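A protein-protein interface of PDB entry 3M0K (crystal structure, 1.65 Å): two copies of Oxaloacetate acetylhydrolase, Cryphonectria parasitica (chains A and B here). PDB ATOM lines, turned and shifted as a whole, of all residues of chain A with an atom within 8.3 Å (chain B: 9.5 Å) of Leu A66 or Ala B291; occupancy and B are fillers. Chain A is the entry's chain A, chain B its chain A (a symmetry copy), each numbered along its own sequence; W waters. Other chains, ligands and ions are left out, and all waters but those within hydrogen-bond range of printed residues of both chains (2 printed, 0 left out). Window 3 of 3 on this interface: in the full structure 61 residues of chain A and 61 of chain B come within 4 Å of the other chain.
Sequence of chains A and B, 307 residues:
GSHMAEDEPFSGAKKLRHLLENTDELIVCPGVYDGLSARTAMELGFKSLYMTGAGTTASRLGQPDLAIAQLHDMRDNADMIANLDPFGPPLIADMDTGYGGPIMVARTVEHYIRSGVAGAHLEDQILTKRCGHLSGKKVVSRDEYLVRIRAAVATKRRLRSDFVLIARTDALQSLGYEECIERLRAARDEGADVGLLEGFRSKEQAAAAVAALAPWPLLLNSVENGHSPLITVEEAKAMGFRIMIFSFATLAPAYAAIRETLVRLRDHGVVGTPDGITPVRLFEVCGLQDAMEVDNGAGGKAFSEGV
The guanidinium group (NH2) of Arg B39 sits close to the side-chain amide nitrogen (NE2) of Gln A63, 3.4 Å away. The backbone nitrogen (N) of Pro A64 lies close to the backbone carbonyl oxygen (O) of Cys B286.
O of Thr A57 is in hydrogen-bond range of N of Gln A63, 3.3 Å away. O of Gln A63 lies within hydrogen-bond range of N of Ala A58. O of Asp A65 sits at hydrogen-bond distance from N of Cys A131 (3.1 Å). O of Phe B283 is in hydrogen-bond range of N of Leu B288, 2.9 Å away.
CB of Ala A58 touches SG of Cys B286 (3.9 Å). CA of Gln A63 touches O of Cys B286, at 3.3 Å. CB of Asp A65 touches CE1 of Phe B283, 3.6 Å away. Leu A66 touches Leu B288. CB of Ala B291 touches CD1 of Leu A66, at 3.7 Å. Cys A131 touches Phe B283.
Of chain B, only Leu B288 and Ala B291 come within 4 Å of Leu A66. Of chain A, only Leu A66 comes within 4 Å of Ala B291. Asp A65 touches one residue of chain B. No residue of chain B comes within 4 Å of Ala A67. Printed residues of chain A within 4 Å of Arg B39: Gln A63 (3.4 Å). Of the printed residues of chain B, Cys A131 touches Phe B283. Of the printed residues of chain A, Cys B286 touches Ala A58 (3.9 Å), Gln A63 (3.3 Å) and Pro A64 (2.9 Å). Gln B289 touches none of the printed residues of chain A. The nearest residue of chain B that does not touch Leu A66 is Met B292 (5.3 Å). The nearest residue of chain A that does not touch Ala B291 is Pro A64 (4.2 Å).
Of the 18 printed residues of chain B, 5 touch a printed residue of chain A. Hydrophobic or aromatic side chains of chain B within 4 Å of the printed part of chain A: Phe B283, Leu B288 and Ala B291. Of the 19 printed residues of chain A, 6 touch a printed residue of chain B. Along chain A the printed residues that touch a printed residue of chain B span positions 58 to 131.
No position is printed for both chains. Of the 8 pairs that touch across the chains among the printed residues, none has its exchanged pair printed and touching as well.
Water W2 lies within hydrogen-bond range of the backbone carbonyl oxygen of Leu B84, the side-chain amide nitrogen of Gln A63 and the guanidinium group of Arg B39. Water W1 bridges OE1 of Gln A63 (2.7 Å) and O of Gly B287 (2.9 Å).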
ATOM      1  N   GLY A  53      17.203  19.475   6.558  1.00  0.00           N
ATOM      2  CA  GLY A  53      15.860  19.360   6.019  1.00  0.00           C
ATOM      3  C   GLY A  53      15.848  19.526   4.511  1.00  0.00           C
ATOM      4  O   GLY A  53      15.175  18.778   3.807  1.00  0.00           O
ATOM      5  N   ALA A  54      16.574  20.525   4.013  1.00  0.00           N
ATOM      6  CA  ALA A  54      16.679  20.730   2.574  1.00  0.00           C
ATOM      7  C   ALA A  54      17.238  19.483   1.903  1.00  0.00           C
ATOM      8  O   ALA A  54      16.727  19.049   0.865  1.00  0.00           O
ATOM      9  CB  ALA A  54      17.545  21.938   2.261  1.00  0.00           C
ATOM     10  N   THR A  57      14.757  16.573   1.961  1.00  0.00           N
ATOM     11  CA  THR A  57      13.712  16.778   0.965  1.00  0.00           C
ATOM     12  C   THR A  57      14.215  16.487  -0.455  1.00  0.00           C
ATOM     13  O   THR A  57      13.538  15.823  -1.247  1.00  0.00           O
ATOM     14  CB  THR A  57      13.158  18.201   1.046  1.00  0.00           C
ATOM     15  OG1 THR A  57      12.775  18.487   2.401  1.00  0.00           O
ATOM     16  CG2 THR A  57      11.948  18.336   0.147  1.00  0.00           C
ATOM     17  N   ALA A  58      15.408  16.973  -0.774  1.00  0.00           N
ATOM     18  CA  ALA A  58      15.986  16.730  -2.096  1.00  0.00           C
ATOM     19  C   ALA A  58      16.209  15.245  -2.351  1.00  0.00           C
ATOM     20  O   ALA A  58      15.863  14.733  -3.419  1.00  0.00           O
ATOM     21  CB  ALA A  58      17.298  17.502  -2.255  1.00  0.00           C
ATOM     22  N   GLN A  63      12.488  16.981  -4.116  1.00  0.00           N
ATOM     23  CA  GLN A  63      11.761  18.244  -4.125  1.00  0.00           C
ATOM     24  C   GLN A  63      12.552  19.370  -3.462  1.00  0.00           C
ATOM     25  O   GLN A  63      13.505  19.124  -2.724  1.00  0.00           O
ATOM     26  CB  GLN A  63      10.419  18.067  -3.395  1.00  0.00           C
ATOM     27  CG  GLN A  63       9.530  17.025  -4.034  1.00  0.00           C
ATOM     28  CD  GLN A  63       9.002  17.461  -5.381  1.00  0.00           C
ATOM     29  OE1 GLN A  63       8.866  18.650  -5.643  1.00  0.00           O
ATOM     30  NE2 GLN A  63       8.694  16.496  -6.244  1.00  0.00           N
ATOM     31  N   PRO A  64      12.150  20.614  -3.723  1.00  0.00           N
ATOM     32  CA  PRO A  64      12.788  21.779  -3.109  1.00  0.00           C
ATOM     33  C   PRO A  64      12.358  21.961  -1.648  1.00  0.00           C
ATOM     34  O   PRO A  64      11.356  21.399  -1.219  1.00  0.00           O
ATOM     35  CB  PRO A  64      12.260  22.930  -3.957  1.00  0.00           C
ATOM     36  CG  PRO A  64      10.935  22.451  -4.420  1.00  0.00           C
ATOM     37  CD  PRO A  64      11.142  21.009  -4.727  1.00  0.00           C
ATOM     38  N   ASP A  65      13.115  22.756  -0.905  1.00  0.00           N
ATOM     39  CA  ASP A  65      12.897  22.917   0.531  1.00  0.00           C
ATOM     40  C   ASP A  65      11.740  23.883   0.790  1.00  0.00           C
ATOM     41  O   ASP A  65      11.944  25.008   1.257  1.00  0.00           O
ATOM     42  CB  ASP A  65      14.188  23.421   1.175  1.00  0.00           C
ATOM     43  CG  ASP A  65      14.146  23.387   2.688  1.00  0.00           C
ATOM     44  OD1 ASP A  65      13.364  22.601   3.256  1.00  0.00           O
ATOM     45  OD2 ASP A  65      14.913  24.153   3.302  1.00  0.00           O
ATOM     46  N   LEU A  66      10.524  23.441   0.476  1.00  0.00           N
ATOM     47  CA  LEU A  66       9.347  24.299   0.549  1.00  0.00           C
ATOM     48  C   LEU A  66       8.244  23.668   1.396  1.00  0.00           C
ATOM     49  O   LEU A  66       7.080  23.627   0.984  1.00  0.00           O
ATOM     50  CB  LEU A  66       8.813  24.598  -0.857  1.00  0.00           C
ATOM     51  CG  LEU A  66       9.767  25.340  -1.802  1.00  0.00           C
ATOM     52  CD1 LEU A  66       9.156  25.495  -3.186  1.00  0.00           C
ATOM     53  CD2 LEU A  66      10.125  26.689  -1.227  1.00  0.00           C
ATOM     54  N   ALA A  67       8.617  23.152   2.562  1.00  0.00           N
ATOM     55  CA  ALA A  67       7.650  22.557   3.484  1.00  0.00           C
ATOM     56  C   ALA A  67       6.937  21.356   2.872  1.00  0.00           C
ATOM     57  O   ALA A  67       5.757  21.102   3.139  1.00  0.00           O
ATOM     58  CB  ALA A  67       6.642  23.610   3.953  1.00  0.00           C
ATOM     59  N   ILE A  68       7.671  20.604   2.066  1.00  0.00           N
ATOM     60  CA  ILE A  68       7.129  19.443   1.379  1.00  0.00           C
ATOM     61  C   ILE A  68       7.379  18.173   2.190  1.00  0.00           C
ATOM     62  O   ILE A  68       6.499  17.318   2.320  1.00  0.00           O
ATOM     63  CB  ILE A  68       7.743  19.326  -0.026  1.00  0.00           C
ATOM     64  CG1 ILE A  68       7.213  20.458  -0.926  1.00  0.00           C
ATOM     65  CG2 ILE A  68       7.459  17.953  -0.612  1.00  0.00           C
ATOM     66  CD1 ILE A  68       7.901  20.572  -2.271  1.00  0.00           C
ATOM     67  N   ALA A  69       8.588  18.052   2.728  1.00  0.00           N
ATOM     68  CA  ALA A  69       8.875  17.013   3.699  1.00  0.00           C
ATOM     69  C   ALA A  69       8.115  17.353   4.975  1.00  0.00           C
ATOM     70  O   ALA A  69       8.075  18.507   5.399  1.00  0.00           O
ATOM     71  CB  ALA A  69      10.379  16.921   3.968  1.00  0.00           C
ATOM     72  N   GLN A  70       7.484  16.345   5.561  1.00  0.00           N
ATOM     73  CA  GLN A  70       6.701  16.544   6.771  1.00  0.00           C
ATOM     74  C   GLN A  70       7.251  15.624   7.842  1.00  0.00           C
ATOM     75  O   GLN A  70       8.295  15.014   7.647  1.00  0.00           O
ATOM     76  CB  GLN A  70       5.237  16.235   6.486  1.00  0.00           C
ATOM     77  CG  GLN A  70       4.676  17.101   5.366  1.00  0.00           C
ATOM     78  CD  GLN A  70       3.168  17.064   5.311  1.00  0.00           C
ATOM     79  OE1 GLN A  70       2.573  16.018   5.068  1.00  0.00           O
ATOM     80  NE2 GLN A  70       2.541  18.211   5.531  1.00  0.00           N
ATOM     81  N   ASP A  96      12.315  21.873  11.444  1.00  0.00           N
ATOM     82  CA  ASP A  96      11.519  22.893  10.787  1.00  0.00           C
ATOM     83  C   ASP A  96      10.655  23.661  11.776  1.00  0.00           C
ATOM     84  O   ASP A  96      11.170  24.194  12.761  1.00  0.00           O
ATOM     85  CB  ASP A  96      10.684  22.247   9.684  1.00  0.00           C
ATOM     86  CG  ASP A  96      11.550  21.720   8.563  1.00  0.00           C
ATOM     87  OD1 ASP A  96      12.039  22.547   7.767  1.00  0.00           O
ATOM     88  OD2 ASP A  96      11.750  20.491   8.493  1.00  0.00           O
ATOM     89  N   GLN A 125       9.436  30.344  11.356  1.00  0.00           N
ATOM     90  CA  GLN A 125       8.817  30.577  10.058  1.00  0.00           C
ATOM     91  C   GLN A 125       7.349  30.183  10.075  1.00  0.00           C
ATOM     92  O   GLN A 125       6.933  29.335  10.866  1.00  0.00           O
ATOM     93  CB  GLN A 125       9.541  29.793   8.962  1.00  0.00           C
ATOM     94  CG  GLN A 125      10.950  30.260   8.716  1.00  0.00           C
ATOM     95  CD  GLN A 125      11.503  29.740   7.408  1.00  0.00           C
ATOM     96  OE1 GLN A 125      12.641  29.287   7.342  1.00  0.00           O
ATOM     97  NE2 GLN A 125      10.690  29.789   6.361  1.00  0.00           N
ATOM     98  N   LEU A 127       4.185  28.162   8.822  1.00  0.00           N
ATOM     99  CA  LEU A 127       4.175  26.741   8.490  1.00  0.00           C
ATOM    100  C   LEU A 127       4.538  26.485   7.028  1.00  0.00           C
ATOM    101  O   LEU A 127       5.278  25.548   6.716  1.00  0.00           O
ATOM    102  CB  LEU A 127       2.825  26.111   8.842  1.00  0.00           C
ATOM    103  CG  LEU A 127       2.533  26.063  10.345  1.00  0.00           C
ATOM    104  CD1 LEU A 127       1.163  25.460  10.622  1.00  0.00           C
ATOM    105  CD2 LEU A 127       3.626  25.291  11.076  1.00  0.00           C
ATOM    106  N   THR A 128       4.022  27.317   6.135  1.00  0.00           N
ATOM    107  CA  THR A 128       4.412  27.247   4.735  1.00  0.00           C
ATOM    108  C   THR A 128       5.793  27.884   4.576  1.00  0.00           C
ATOM    109  O   THR A 128       5.942  28.934   3.948  1.00  0.00           O
ATOM    110  CB  THR A 128       3.382  27.943   3.836  1.00  0.00           C
ATOM    111  OG1 THR A 128       3.264  29.318   4.221  1.00  0.00           O
ATOM    112  CG2 THR A 128       2.023  27.275   3.983  1.00  0.00           C
ATOM    113  N   LYS A 129       6.798  27.231   5.155  1.00  0.00           N
ATOM    114  CA  LYS A 129       8.161  27.762   5.226  1.00  0.00           C
ATOM    115  C   LYS A 129       8.977  27.589   3.943  1.00  0.00           C
ATOM    116  O   LYS A 129       8.462  27.166   2.906  1.00  0.00           O
ATOM    117  CB  LYS A 129       8.918  27.108   6.388  1.00  0.00           C
ATOM    118  CG  LYS A 129       9.021  25.592   6.273  1.00  0.00           C
ATOM    119  N   ARG A 130      10.262  27.917   4.038  1.00  0.00           N
ATOM    120  CA  ARG A 130      11.181  27.813   2.913  1.00  0.00           C
ATOM    121  C   ARG A 130      12.624  27.921   3.396  1.00  0.00           C
ATOM    122  O   ARG A 130      12.881  28.370   4.517  1.00  0.00           O
ATOM    123  N   CYS A 131      13.571  27.395   2.501  1.00  0.00           N
ATOM    124  CA  CYS A 131      15.023  27.556   2.884  1.00  0.00           C
ATOM    125  C   CYS A 131      15.344  28.984   3.434  1.00  0.00           C
ATOM    126  O   CYS A 131      14.900  30.109   2.862  1.00  0.00           O
ATOM    127  CB  CYS A 131      15.894  27.316   1.657  1.00  0.00           C
ATOM    128  SG  CYS A 131      17.678  27.835   1.650  1.00  0.00           S
ATOM    129  N   ARG B  39      17.040  13.523 -10.217  1.00  0.00           N
ATOM    130  CA  ARG B  39      16.768  14.847 -10.776  1.00  0.00           C
ATOM    131  C   ARG B  39      17.901  15.284 -11.697  1.00  0.00           C
ATOM    132  O   ARG B  39      17.657  15.940 -12.706  1.00  0.00           O
ATOM    133  CB  ARG B  39      16.544  15.886  -9.670  1.00  0.00           C
ATOM    134  CG  ARG B  39      15.167  15.824  -9.002  1.00  0.00           C
ATOM    135  CD  ARG B  39      14.043  16.328  -9.912  1.00  0.00           C
ATOM    136  NE  ARG B  39      12.840  16.633  -9.127  1.00  0.00           N
ATOM    137  CZ  ARG B  39      11.710  17.123  -9.621  1.00  0.00           C
ATOM    138  NH1 ARG B  39      11.592  17.367 -10.921  1.00  0.00           N
ATOM    139  NH2 ARG B  39      10.684  17.359  -8.804  1.00  0.00           N
ATOM    140  N   LEU B  84       8.701  11.994 -10.315  1.00  0.00           N
ATOM    141  CA  LEU B  84       9.180  13.354 -10.129  1.00  0.00           C
ATOM    142  C   LEU B  84       8.634  14.226 -11.246  1.00  0.00           C
ATOM    143  O   LEU B  84       8.292  15.386 -11.030  1.00  0.00           O
ATOM    144  CB  LEU B  84      10.704  13.386 -10.110  1.00  0.00           C
ATOM    145  CG  LEU B  84      11.287  12.668  -8.901  1.00  0.00           C
ATOM    146  CD1 LEU B  84      12.807  12.636  -9.004  1.00  0.00           C
ATOM    147  CD2 LEU B  84      10.825  13.384  -7.629  1.00  0.00           C
ATOM    148  N   PHE B 283      17.778  23.554  -5.658  1.00  0.00           N
ATOM    149  CA  PHE B 283      16.321  23.553  -5.636  1.00  0.00           C
ATOM    150  C   PHE B 283      15.774  23.550  -7.062  1.00  0.00           C
ATOM    151  O   PHE B 283      14.783  22.891  -7.363  1.00  0.00           O
ATOM    152  CB  PHE B 283      15.772  24.754  -4.864  1.00  0.00           C
ATOM    153  CG  PHE B 283      16.175  24.784  -3.411  1.00  0.00           C
ATOM    154  CD1 PHE B 283      16.344  23.606  -2.703  1.00  0.00           C
ATOM    155  CD2 PHE B 283      16.375  25.998  -2.748  1.00  0.00           C
ATOM    156  CE1 PHE B 283      16.721  23.630  -1.351  1.00  0.00           C
ATOM    157  CE2 PHE B 283      16.739  26.029  -1.404  1.00  0.00           C
ATOM    158  CZ  PHE B 283      16.916  24.843  -0.706  1.00  0.00           C
ATOM    159  N   GLU B 284      16.436  24.290  -7.943  1.00  0.00           N
ATOM    160  CA  GLU B 284      16.030  24.324  -9.340  1.00  0.00           C
ATOM    161  C   GLU B 284      16.128  22.940  -9.956  1.00  0.00           C
ATOM    162  O   GLU B 284      15.261  22.522 -10.717  1.00  0.00           O
ATOM    163  CB  GLU B 284      16.893  25.306 -10.118  1.00  0.00           C
ATOM    164  CG  GLU B 284      16.620  26.753  -9.755  1.00  0.00           C
ATOM    165  CD  GLU B 284      17.578  27.700 -10.439  1.00  0.00           C
ATOM    166  OE1 GLU B 284      18.679  27.253 -10.834  1.00  0.00           O
ATOM    167  OE2 GLU B 284      17.230  28.890 -10.582  1.00  0.00           O
ATOM    168  N   CYS B 286      15.872  20.275  -8.395  1.00  0.00           N
ATOM    169  CA  CYS B 286      14.871  19.450  -7.735  1.00  0.00           C
ATOM    170  C   CYS B 286      13.450  20.001  -7.826  1.00  0.00           C
ATOM    171  O   CYS B 286      12.654  19.775  -6.929  1.00  0.00           O
ATOM    172  CB  CYS B 286      15.257  19.224  -6.272  1.00  0.00           C
ATOM    173  SG  CYS B 286      16.735  18.243  -6.088  1.00  0.00           S
ATOM    174  N   GLY B 287      13.146  20.736  -8.892  1.00  0.00           N
ATOM    175  CA  GLY B 287      11.768  21.077  -9.215  1.00  0.00           C
ATOM    176  C   GLY B 287      11.240  22.382  -8.650  1.00  0.00           C
ATOM    177  O   GLY B 287      10.030  22.538  -8.481  1.00  0.00           O
ATOM    178  N   LEU B 288      12.126  23.328  -8.363  1.00  0.00           N
ATOM    179  CA  LEU B 288      11.681  24.600  -7.808  1.00  0.00           C
ATOM    180  C   LEU B 288      10.690  25.298  -8.746  1.00  0.00           C
ATOM    181  O   LEU B 288       9.673  25.833  -8.310  1.00  0.00           O
ATOM    182  CB  LEU B 288      12.874  25.516  -7.545  1.00  0.00           C
ATOM    183  CG  LEU B 288      12.514  26.890  -6.993  1.00  0.00           C
ATOM    184  CD1 LEU B 288      11.900  26.736  -5.617  1.00  0.00           C
ATOM    185  CD2 LEU B 288      13.756  27.769  -6.943  1.00  0.00           C
ATOM    186  N   GLN B 289      11.000  25.300 -10.038  1.00  0.00           N
ATOM    187  CA  GLN B 289      10.166  26.008 -11.002  1.00  0.00           C
ATOM    188  C   GLN B 289       8.743  25.466 -11.013  1.00  0.00           C
ATOM    189  O   GLN B 289       7.788  26.229 -10.945  1.00  0.00           O
ATOM    190  CB  GLN B 289      10.767  25.938 -12.403  1.00  0.00           C
ATOM    191  CG  GLN B 289       9.997  26.745 -13.444  1.00  0.00           C
ATOM    192  CD  GLN B 289       9.795  28.199 -13.043  1.00  0.00           C
ATOM    193  OE1 GLN B 289       8.855  28.853 -13.500  1.00  0.00           O
ATOM    194  NE2 GLN B 289      10.679  28.713 -12.191  1.00  0.00           N
ATOM    195  N   ASP B 290       8.611  24.148 -11.106  1.00  0.00           N
ATOM    196  CA  ASP B 290       7.302  23.508 -11.032  1.00  0.00           C
ATOM    197  C   ASP B 290       6.550  23.969  -9.789  1.00  0.00           C
ATOM    198  O   ASP B 290       5.382  24.335  -9.868  1.00  0.00           O
ATOM    199  CB  ASP B 290       7.448  21.992 -10.979  1.00  0.00           C
ATOM    200  CG  ASP B 290       7.833  21.397 -12.310  1.00  0.00           C
ATOM    201  OD1 ASP B 290       7.735  22.099 -13.337  1.00  0.00           O
ATOM    202  OD2 ASP B 290       8.230  20.217 -12.325  1.00  0.00           O
ATOM    203  N   ALA B 291       7.225  23.958  -8.646  1.00  0.00           N
ATOM    204  CA  ALA B 291       6.594  24.335  -7.388  1.00  0.00           C
ATOM    205  C   ALA B 291       6.132  25.788  -7.378  1.00  0.00           C
ATOM    206  O   ALA B 291       5.043  26.102  -6.911  1.00  0.00           O
ATOM    207  CB  ALA B 291       7.534  24.076  -6.229  1.00  0.00           C
ATOM    208  N   MET B 292       6.978  26.683  -7.874  1.00  0.00           N
ATOM    209  CA  MET B 292       6.616  28.092  -7.919  1.00  0.00           C
ATOM    210  C   MET B 292       5.437  28.307  -8.863  1.00  0.00           C
ATOM    211  O   MET B 292       4.555  29.115  -8.582  1.00  0.00           O
ATOM    212  CB  MET B 292       7.816  28.942  -8.335  1.00  0.00           C
ATOM    213  CG  MET B 292       8.872  29.075  -7.254  1.00  0.00           C
ATOM    214  SD  MET B 292      10.199  30.200  -7.731  1.00  0.00           S
ATOM    215  CE  MET B 292      10.577  30.942  -6.141  1.00  0.00           C
ATOM    216  N   GLU B 293       5.428  27.576  -9.973  1.00  0.00           N
ATOM    217  CA  GLU B 293       4.318  27.621 -10.924  1.00  0.00           C
ATOM    218  C   GLU B 293       3.017  27.193 -10.260  1.00  0.00           C
ATOM    219  O   GLU B 293       1.962  27.776 -10.501  1.00  0.00           O
ATOM    220  CB  GLU B 293       4.579  26.706 -12.125  1.00  0.00           C
ATOM    221  CG  GLU B 293       5.712  27.138 -13.051  1.00  0.00           C
ATOM    222  CD  GLU B 293       5.908  26.162 -14.203  1.00  0.00           C
ATOM    223  OE1 GLU B 293       4.916  25.832 -14.883  1.00  0.00           O
ATOM    224  OE2 GLU B 293       7.054  25.718 -14.429  1.00  0.00           O
ATOM    225  N   VAL B 294       3.085  26.148  -9.443  1.00  0.00           N
ATOM    226  CA  VAL B 294       1.902  25.681  -8.737  1.00  0.00           C
ATOM    227  C   VAL B 294       1.388  26.786  -7.838  1.00  0.00           C
ATOM    228  O   VAL B 294       0.206  27.128  -7.871  1.00  0.00           O
ATOM    229  CB  VAL B 294       2.203  24.432  -7.887  1.00  0.00           C
ATOM    230  CG1 VAL B 294       1.082  24.193  -6.879  1.00  0.00           C
ATOM    231  CG2 VAL B 294       2.402  23.218  -8.785  1.00  0.00           C
ATOM    232  N   ASP B 295       2.285  27.361  -7.047  1.00  0.00           N
ATOM    233  CA  ASP B 295       1.900  28.382  -6.085  1.00  0.00           C
ATOM    234  C   ASP B 295       1.354  29.631  -6.767  1.00  0.00           C
ATOM    235  O   ASP B 295       0.295  30.135  -6.400  1.00  0.00           O
ATOM    236  CB  ASP B 295       3.087  28.760  -5.200  1.00  0.00           C
ATOM    237  CG  ASP B 295       2.680  29.645  -4.045  1.00  0.00           C
ATOM    238  OD1 ASP B 295       2.211  29.102  -3.025  1.00  0.00           O
ATOM    239  OD2 ASP B 295       2.817  30.881  -4.158  1.00  0.00           O
ATOM    240  N   ASN B 296       2.090  30.137  -7.748  1.00  0.00           N
ATOM    241  CA  ASN B 296       1.657  31.321  -8.473  1.00  0.00           C
ATOM    242  C   ASN B 296       0.338  31.060  -9.185  1.00  0.00           C
ATOM    243  O   ASN B 296      -0.578  31.876  -9.124  1.00  0.00           O
ATOM    244  CB  ASN B 296       2.723  31.756  -9.478  1.00  0.00           C
ATOM    245  CG  ASN B 296       2.344  33.031 -10.214  1.00  0.00           C
ATOM    246  OD1 ASN B 296       2.089  34.068  -9.597  1.00  0.00           O
ATOM    247  ND2 ASN B 296       2.305  32.959 -11.542  1.00  0.00           N
ATOM    248  N   GLY B 297       0.244  29.915  -9.852  1.00  0.00           N
ATOM    249  CA  GLY B 297      -0.959  29.551 -10.576  1.00  0.00           C
ATOM    250  C   GLY B 297      -2.198  29.431  -9.703  1.00  0.00           C
ATOM    251  O   GLY B 297      -3.317  29.665 -10.166  1.00  0.00           O
ATOM    252  N   ALA B 298      -2.012  29.055  -8.443  1.00  0.00           N
ATOM    253  CA  ALA B 298      -3.140  28.839  -7.542  1.00  0.00           C
ATOM    254  C   ALA B 298      -3.659  30.150  -6.972  1.00  0.00           C
ATOM    255  O   ALA B 298      -4.626  30.167  -6.214  1.00  0.00           O
ATOM    256  CB  ALA B 298      -2.753  27.899  -6.419  1.00  0.00           C
ATOM    257  N   GLY B 300      -1.746  32.126  -5.241  1.00  0.00           N
ATOM    258  CA  GLY B 300      -0.891  32.437  -4.112  1.00  0.00           C
ATOM    259  C   GLY B 300       0.147  33.480  -4.493  1.00  0.00           C
ATOM    260  O   GLY B 300       0.470  33.656  -5.672  1.00  0.00           O
HETATM  261  O   HOH W   1       8.173  20.530  -7.500  1.00  0.00           O
HETATM  262  O   HOH W   2       7.463  16.704  -8.940  1.00  0.00           O
